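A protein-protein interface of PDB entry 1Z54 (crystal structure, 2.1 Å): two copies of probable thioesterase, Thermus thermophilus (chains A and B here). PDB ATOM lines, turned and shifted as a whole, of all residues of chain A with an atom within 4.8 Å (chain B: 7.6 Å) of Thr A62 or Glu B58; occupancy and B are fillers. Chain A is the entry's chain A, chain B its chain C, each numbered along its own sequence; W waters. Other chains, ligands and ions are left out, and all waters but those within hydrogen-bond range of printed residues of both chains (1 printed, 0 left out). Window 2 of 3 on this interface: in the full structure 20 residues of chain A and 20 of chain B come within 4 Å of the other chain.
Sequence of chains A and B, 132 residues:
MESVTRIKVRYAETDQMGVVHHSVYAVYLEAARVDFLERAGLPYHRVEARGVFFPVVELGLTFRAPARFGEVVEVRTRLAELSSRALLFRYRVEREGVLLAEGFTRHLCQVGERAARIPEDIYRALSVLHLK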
ATOM      1  N   GLY A  60       0.967  16.770  25.565  1.00  0.00           N
ATOM      2  CA  GLY A  60       1.938  15.767  25.944  1.00  0.00           C
ATOM      3  C   GLY A  60       1.528  15.161  27.266  1.00  0.00           C
ATOM      4  O   GLY A  60       1.244  15.884  28.219  1.00  0.00           O
ATOM      5  N   LEU A  61       1.485  13.835  27.327  1.00  0.00           N
ATOM      6  CA  LEU A  61       1.101  13.155  28.550  1.00  0.00           C
ATOM      7  C   LEU A  61       1.917  11.907  28.808  1.00  0.00           C
ATOM      8  O   LEU A  61       2.151  11.102  27.904  1.00  0.00           O
ATOM      9  CB  LEU A  61      -0.388  12.783  28.516  1.00  0.00           C
ATOM     10  CG  LEU A  61      -1.376  13.798  29.096  1.00  0.00           C
ATOM     11  CD1 LEU A  61      -2.746  13.586  28.485  1.00  0.00           C
ATOM     12  CD2 LEU A  61      -1.432  13.661  30.620  1.00  0.00           C
ATOM     13  N   THR A  62       2.350  11.758  30.055  1.00  0.00           N
ATOM     14  CA  THR A  62       3.109  10.585  30.465  1.00  0.00           C
ATOM     15  C   THR A  62       2.301   9.942  31.577  1.00  0.00           C
ATOM     16  O   THR A  62       2.046  10.557  32.613  1.00  0.00           O
ATOM     17  CB  THR A  62       4.514  10.961  30.973  1.00  0.00           C
ATOM     18  OG1 THR A  62       5.249  11.570  29.905  1.00  0.00           O
ATOM     19  CG2 THR A  62       5.265   9.720  31.464  1.00  0.00           C
ATOM     20  N   PHE A  63       1.882   8.707  31.334  1.00  0.00           N
ATOM     21  CA  PHE A  63       1.066   7.956  32.275  1.00  0.00           C
ATOM     22  C   PHE A  63       1.959   7.074  33.142  1.00  0.00           C
ATOM     23  O   PHE A  63       2.627   6.172  32.636  1.00  0.00           O
ATOM     24  CB  PHE A  63       0.056   7.112  31.490  1.00  0.00           C
ATOM     25  CG  PHE A  63      -0.747   7.907  30.487  1.00  0.00           C
ATOM     26  CD1 PHE A  63      -1.909   8.573  30.871  1.00  0.00           C
ATOM     27  CD2 PHE A  63      -0.326   8.005  29.155  1.00  0.00           C
ATOM     28  CE1 PHE A  63      -2.648   9.327  29.947  1.00  0.00           C
ATOM     29  CE2 PHE A  63      -1.056   8.757  28.223  1.00  0.00           C
ATOM     30  CZ  PHE A  63      -2.220   9.419  28.621  1.00  0.00           C
ATOM     31  N   ARG A  64       1.963   7.347  34.446  1.00  0.00           N
ATOM     32  CA  ARG A  64       2.788   6.609  35.404  1.00  0.00           C
ATOM     33  C   ARG A  64       2.007   5.537  36.169  1.00  0.00           C
ATOM     34  O   ARG A  64       2.504   4.431  36.385  1.00  0.00           O
ATOM     35  CB  ARG A  64       3.399   7.583  36.415  1.00  0.00           C
ATOM     36  CG  ARG A  64       4.105   8.797  35.809  1.00  0.00           C
ATOM     37  CD  ARG A  64       5.406   8.410  35.128  1.00  0.00           C
ATOM     38  NE  ARG A  64       6.232   9.583  34.842  1.00  0.00           N
ATOM     39  CZ  ARG A  64       7.474   9.524  34.366  1.00  0.00           C
ATOM     40  NH1 ARG A  64       8.154  10.639  34.134  1.00  0.00           N
ATOM     41  NH2 ARG A  64       8.038   8.345  34.120  1.00  0.00           N
ATOM     42  N   LEU A 100      -0.032  10.069  39.088  1.00  0.00           N
ATOM     43  CA  LEU A 100      -0.688   9.169  38.149  1.00  0.00           C
ATOM     44  C   LEU A 100      -0.205   9.411  36.737  1.00  0.00           C
ATOM     45  O   LEU A 100      -0.007   8.475  35.959  1.00  0.00           O
ATOM     46  CB  LEU A 100      -2.205   9.345  38.218  1.00  0.00           C
ATOM     47  CG  LEU A 100      -2.792   9.057  39.596  1.00  0.00           C
ATOM     48  CD1 LEU A 100      -4.313   8.976  39.485  1.00  0.00           C
ATOM     49  CD2 LEU A 100      -2.230   7.739  40.137  1.00  0.00           C
ATOM     50  N   ALA A 101      -0.014  10.681  36.411  1.00  0.00           N
ATOM     51  CA  ALA A 101       0.450  11.068  35.094  1.00  0.00           C
ATOM     52  C   ALA A 101       0.849  12.525  35.172  1.00  0.00           C
ATOM     53  O   ALA A 101       0.492  13.224  36.119  1.00  0.00           O
ATOM     54  CB  ALA A 101      -0.663  10.886  34.069  1.00  0.00           C
ATOM     55  N   GLU A 102       1.595  12.983  34.180  1.00  0.00           N
ATOM     56  CA  GLU A 102       2.017  14.374  34.138  1.00  0.00           C
ATOM     57  C   GLU A 102       2.049  14.794  32.683  1.00  0.00           C
ATOM     58  O   GLU A 102       2.319  13.978  31.799  1.00  0.00           O
ATOM     59  CB  GLU A 102       3.396  14.536  34.778  1.00  0.00           C
ATOM     60  CG  GLU A 102       4.474  13.653  34.190  1.00  0.00           C
ATOM     61  CD  GLU A 102       5.711  13.601  35.068  1.00  0.00           C
ATOM     62  OE1 GLU A 102       6.294  14.674  35.344  1.00  0.00           O
ATOM     63  OE2 GLU A 102       6.096  12.487  35.484  1.00  0.00           O
ATOM     64  N   PRO B  55      -0.901  -1.239  26.774  1.00  0.00           N
ATOM     65  CA  PRO B  55      -1.267   0.005  27.463  1.00  0.00           C
ATOM     66  C   PRO B  55      -0.402   1.180  27.011  1.00  0.00           C
ATOM     67  O   PRO B  55       0.758   0.999  26.657  1.00  0.00           O
ATOM     68  CB  PRO B  55      -1.062  -0.346  28.942  1.00  0.00           C
ATOM     69  CG  PRO B  55       0.020  -1.381  28.899  1.00  0.00           C
ATOM     70  CD  PRO B  55      -0.399  -2.243  27.728  1.00  0.00           C
ATOM     71  N   VAL B  56      -0.984   2.377  27.002  1.00  0.00           N
ATOM     72  CA  VAL B  56      -0.269   3.586  26.602  1.00  0.00           C
ATOM     73  C   VAL B  56       0.460   4.170  27.809  1.00  0.00           C
ATOM     74  O   VAL B  56      -0.146   4.367  28.860  1.00  0.00           O
ATOM     75  CB  VAL B  56      -1.235   4.675  26.054  1.00  0.00           C
ATOM     76  CG1 VAL B  56      -0.471   5.964  25.793  1.00  0.00           C
ATOM     77  CG2 VAL B  56      -1.903   4.197  24.773  1.00  0.00           C
ATOM     78  N   VAL B  57       1.756   4.440  27.656  1.00  0.00           N
ATOM     79  CA  VAL B  57       2.556   5.020  28.740  1.00  0.00           C
ATOM     80  C   VAL B  57       2.890   6.482  28.442  1.00  0.00           C
ATOM     81  O   VAL B  57       3.236   7.246  29.342  1.00  0.00           O
ATOM     82  CB  VAL B  57       3.869   4.234  28.965  1.00  0.00           C
ATOM     83  CG1 VAL B  57       3.546   2.804  29.365  1.00  0.00           C
ATOM     84  CG2 VAL B  57       4.724   4.250  27.696  1.00  0.00           C
ATOM     85  N   GLU B  58       2.798   6.869  27.174  1.00  0.00           N
ATOM     86  CA  GLU B  58       3.048   8.254  26.792  1.00  0.00           C
ATOM     87  C   GLU B  58       2.352   8.591  25.486  1.00  0.00           C
ATOM     88  O   GLU B  58       2.235   7.753  24.587  1.00  0.00           O
ATOM     89  CB  GLU B  58       4.550   8.543  26.657  1.00  0.00           C
ATOM     90  CG  GLU B  58       4.848  10.021  26.385  1.00  0.00           C
ATOM     91  CD  GLU B  58       6.327  10.318  26.224  1.00  0.00           C
ATOM     92  OE1 GLU B  58       6.679  11.503  26.064  1.00  0.00           O
ATOM     93  OE2 GLU B  58       7.135   9.370  26.248  1.00  0.00           O
ATOM     94  N   LEU B  59       1.892   9.835  25.393  1.00  0.00           N
ATOM     95  CA  LEU B  59       1.197  10.331  24.215  1.00  0.00           C
ATOM     96  C   LEU B  59       1.692  11.723  23.851  1.00  0.00           C
ATOM     97  O   LEU B  59       1.976  12.542  24.726  1.00  0.00           O
ATOM     98  CB  LEU B  59      -0.308  10.397  24.488  1.00  0.00           C
ATOM     99  CG  LEU B  59      -1.102  11.314  23.555  1.00  0.00           C
ATOM    100  CD1 LEU B  59      -1.081  10.744  22.146  1.00  0.00           C
ATOM    101  CD2 LEU B  59      -2.527  11.453  24.050  1.00  0.00           C
ATOM    102  N   GLY B  60       1.785  11.984  22.554  1.00  0.00           N
ATOM    103  CA  GLY B  60       2.219  13.286  22.092  1.00  0.00           C
ATOM    104  C   GLY B  60       1.440  13.672  20.850  1.00  0.00           C
ATOM    105  O   GLY B  60       1.227  12.844  19.959  1.00  0.00           O
ATOM    106  N   LEU B  87       6.767  -0.398  22.291  1.00  0.00           N
ATOM    107  CA  LEU B  87       6.410  -0.004  20.930  1.00  0.00           C
ATOM    108  C   LEU B  87       6.224   1.504  20.881  1.00  0.00           C
ATOM    109  O   LEU B  87       5.821   2.120  21.867  1.00  0.00           O
ATOM    110  CB  LEU B  87       5.075  -0.628  20.495  1.00  0.00           C
ATOM    111  CG  LEU B  87       4.773  -2.123  20.564  1.00  0.00           C
ATOM    112  CD1 LEU B  87       5.779  -2.866  19.732  1.00  0.00           C
ATOM    113  CD2 LEU B  87       4.799  -2.607  22.011  1.00  0.00           C
ATOM    114  N   LEU B  88       6.501   2.091  19.725  1.00  0.00           N
ATOM    115  CA  LEU B  88       6.307   3.521  19.543  1.00  0.00           C
ATOM    116  C   LEU B  88       5.689   3.752  18.174  1.00  0.00           C
ATOM    117  O   LEU B  88       6.330   3.509  17.143  1.00  0.00           O
ATOM    118  CB  LEU B  88       7.635   4.282  19.643  1.00  0.00           C
ATOM    119  CG  LEU B  88       7.548   5.820  19.645  1.00  0.00           C
ATOM    120  CD1 LEU B  88       7.045   6.332  18.313  1.00  0.00           C
ATOM    121  CD2 LEU B  88       6.629   6.281  20.763  1.00  0.00           C
ATOM    122  N   PHE B  89       4.440   4.208  18.166  1.00  0.00           N
ATOM    123  CA  PHE B  89       3.744   4.494  16.919  1.00  0.00           C
ATOM    124  C   PHE B  89       3.782   5.994  16.640  1.00  0.00           C
ATOM    125  O   PHE B  89       3.659   6.810  17.552  1.00  0.00           O
ATOM    126  CB  PHE B  89       2.272   4.070  16.982  1.00  0.00           C
ATOM    127  CG  PHE B  89       2.059   2.592  17.132  1.00  0.00           C
ATOM    128  CD1 PHE B  89       2.012   2.008  18.395  1.00  0.00           C
ATOM    129  CD2 PHE B  89       1.898   1.784  16.009  1.00  0.00           C
ATOM    130  CE1 PHE B  89       1.808   0.640  18.538  1.00  0.00           C
ATOM    131  CE2 PHE B  89       1.695   0.414  16.135  1.00  0.00           C
ATOM    132  CZ  PHE B  89       1.649  -0.163  17.402  1.00  0.00           C
ATOM    133  N   PHE B 104       2.321  10.755  18.441  1.00  0.00           N
ATOM    134  CA  PHE B 104       2.870   9.444  18.712  1.00  0.00           C
ATOM    135  C   PHE B 104       2.284   8.887  19.999  1.00  0.00           C
ATOM    136  O   PHE B 104       1.752   9.626  20.824  1.00  0.00           O
ATOM    137  CB  PHE B 104       4.382   9.569  18.883  1.00  0.00           C
ATOM    138  CG  PHE B 104       4.788  10.291  20.149  1.00  0.00           C
ATOM    139  CD1 PHE B 104       4.907   9.602  21.350  1.00  0.00           C
ATOM    140  CD2 PHE B 104       5.034  11.658  20.138  1.00  0.00           C
ATOM    141  CE1 PHE B 104       5.269  10.264  22.527  1.00  0.00           C
ATOM    142  CE2 PHE B 104       5.397  12.330  21.308  1.00  0.00           C
ATOM    143  CZ  PHE B 104       5.515  11.629  22.505  1.00  0.00           C
ATOM    144  N   THR B 105       2.396   7.577  20.158  1.00  0.00           N
ATOM    145  CA  THR B 105       1.954   6.910  21.364  1.00  0.00           C
ATOM    146  C   THR B 105       3.058   5.911  21.686  1.00  0.00           C
ATOM    147  O   THR B 105       3.590   5.251  20.791  1.00  0.00           O
ATOM    148  CB  THR B 105       0.610   6.157  21.177  1.00  0.00           C
ATOM    149  OG1 THR B 105       0.692   5.292  20.037  1.00  0.00           O
ATOM    150  CG2 THR B 105      -0.543   7.142  20.995  1.00  0.00           C
ATOM    151  N   ARG B 106       3.427   5.829  22.956  1.00  0.00           N
ATOM    152  CA  ARG B 106       4.455   4.897  23.394  1.00  0.00           C
ATOM    153  C   ARG B 106       3.735   3.829  24.205  1.00  0.00           C
ATOM    154  O   ARG B 106       2.854   4.141  25.013  1.00  0.00           O
ATOM    155  CB  ARG B 106       5.495   5.625  24.247  1.00  0.00           C
ATOM    156  CG  ARG B 106       6.694   4.771  24.654  1.00  0.00           C
ATOM    157  CD  ARG B 106       7.866   5.663  25.070  1.00  0.00           C
ATOM    158  NE  ARG B 106       7.574   6.479  26.245  1.00  0.00           N
ATOM    159  CZ  ARG B 106       7.685   6.051  27.498  1.00  0.00           C
ATOM    160  NH1 ARG B 106       7.393   6.864  28.510  1.00  0.00           N
ATOM    161  NH2 ARG B 106       8.104   4.813  27.742  1.00  0.00           N
ATOM    162  N   HIS B 107       4.092   2.570  23.990  1.00  0.00           N
ATOM    163  CA  HIS B 107       3.420   1.492  24.702  1.00  0.00           C
ATOM    164  C   HIS B 107       4.364   0.497  25.348  1.00  0.00           C
ATOM    165  O   HIS B 107       5.493   0.309  24.899  1.00  0.00           O
ATOM    166  CB  HIS B 107       2.515   0.689  23.753  1.00  0.00           C
ATOM    167  CG  HIS B 107       1.497   1.506  23.018  1.00  0.00           C
ATOM    168  ND1 HIS B 107       1.830   2.384  22.007  1.00  0.00           N
ATOM    169  CD2 HIS B 107       0.147   1.535  23.111  1.00  0.00           C
ATOM    170  CE1 HIS B 107       0.728   2.915  21.506  1.00  0.00           C
ATOM    171  NE2 HIS B 107      -0.307   2.417  22.157  1.00  0.00           N
ATOM    172  N   LEU B 108       3.870  -0.142  26.400  1.00  0.00           N
ATOM    173  CA  LEU B 108       4.599  -1.197  27.093  1.00  0.00           C
ATOM    174  C   LEU B 108       3.728  -2.410  26.823  1.00  0.00           C
ATOM    175  O   LEU B 108       2.600  -2.260  26.355  1.00  0.00           O
ATOM    176  CB  LEU B 108       4.654  -0.947  28.604  1.00  0.00           C
ATOM    177  CG  LEU B 108       5.666   0.077  29.117  1.00  0.00           C
ATOM    178  CD1 LEU B 108       5.598   0.118  30.636  1.00  0.00           C
ATOM    179  CD2 LEU B 108       7.073  -0.291  28.657  1.00  0.00           C
HETATM  180  O   HOH W   1       4.538  13.448  25.683  1.00  0.00           O
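Printed residues of chain B that touch a printed residue of chain A: Val B56, Val B57, Glu B58 and Leu B59.
Along chain A the printed residues that touch a printed residue of chain B span positions 60 to 63.
Among the printed residues, pairs that only touch across the chains: Gly A60 with Leu B59 (3.4 Å), Leu A61 with Glu B58 (3.2 Å), Thr A62 with Val B57 (3.5 Å), Thr A62 with Glu B58 (3.9 Å), Phe A63 with Val B56 (3.7 Å) and Phe A63 with Glu B58 (3.9 Å).
Water W1 lies within hydrogen-bond range of the backbone carbonyl oxygen (O) of Leu B59 (2.9 Å), the side-chain carboxylate (OE1) of Glu B58 (2.9 Å) and the backbone NH (N) of Leu A61 (3.5 Å).
Position printed for both chains: 60.
Of the 8 pairs that touch across the chains among the printed residues, none has its exchanged pair printed and touching as well.
N of Phe A63 is in hydrogen-bond range of O of Val B57 (2.8 Å).
The backbone carbonyl oxygen of Leu A61 is in hydrogen-bond range of the backbone NH of Leu B59 (2.8 Å).
The backbone carbonyl oxygen of Glu A102 is in hydrogen-bond range of the backbone NH of Thr A62 (2.8 Å).
OE2 of Glu B58 is in salt-bridge range of NE of Arg B106, 2.9 Å away.
The backbone NH (N) of Val B57 is in hydrogen-bond range of the backbone carbonyl oxygen (O) of Arg B106.
Of the printed residues of chain B, Gly A60 touches Leu B59.
Printed residues of chain A within 4 Å of Val B57: Thr A62 (3.5 Å) and Phe A63 (2.8 Å).
Glu B58 touches just these residues of chain A: Leu A61 (3.2 Å), Thr A62 (3.9 Å) and Phe A63 (3.9 Å).
Printed residues of chain A within 4 Å of Leu B59: Gly A60 and Leu A61.
The nearest printed residue of chain A that does not touch Val B56 is Leu A61 (6.1 Å).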
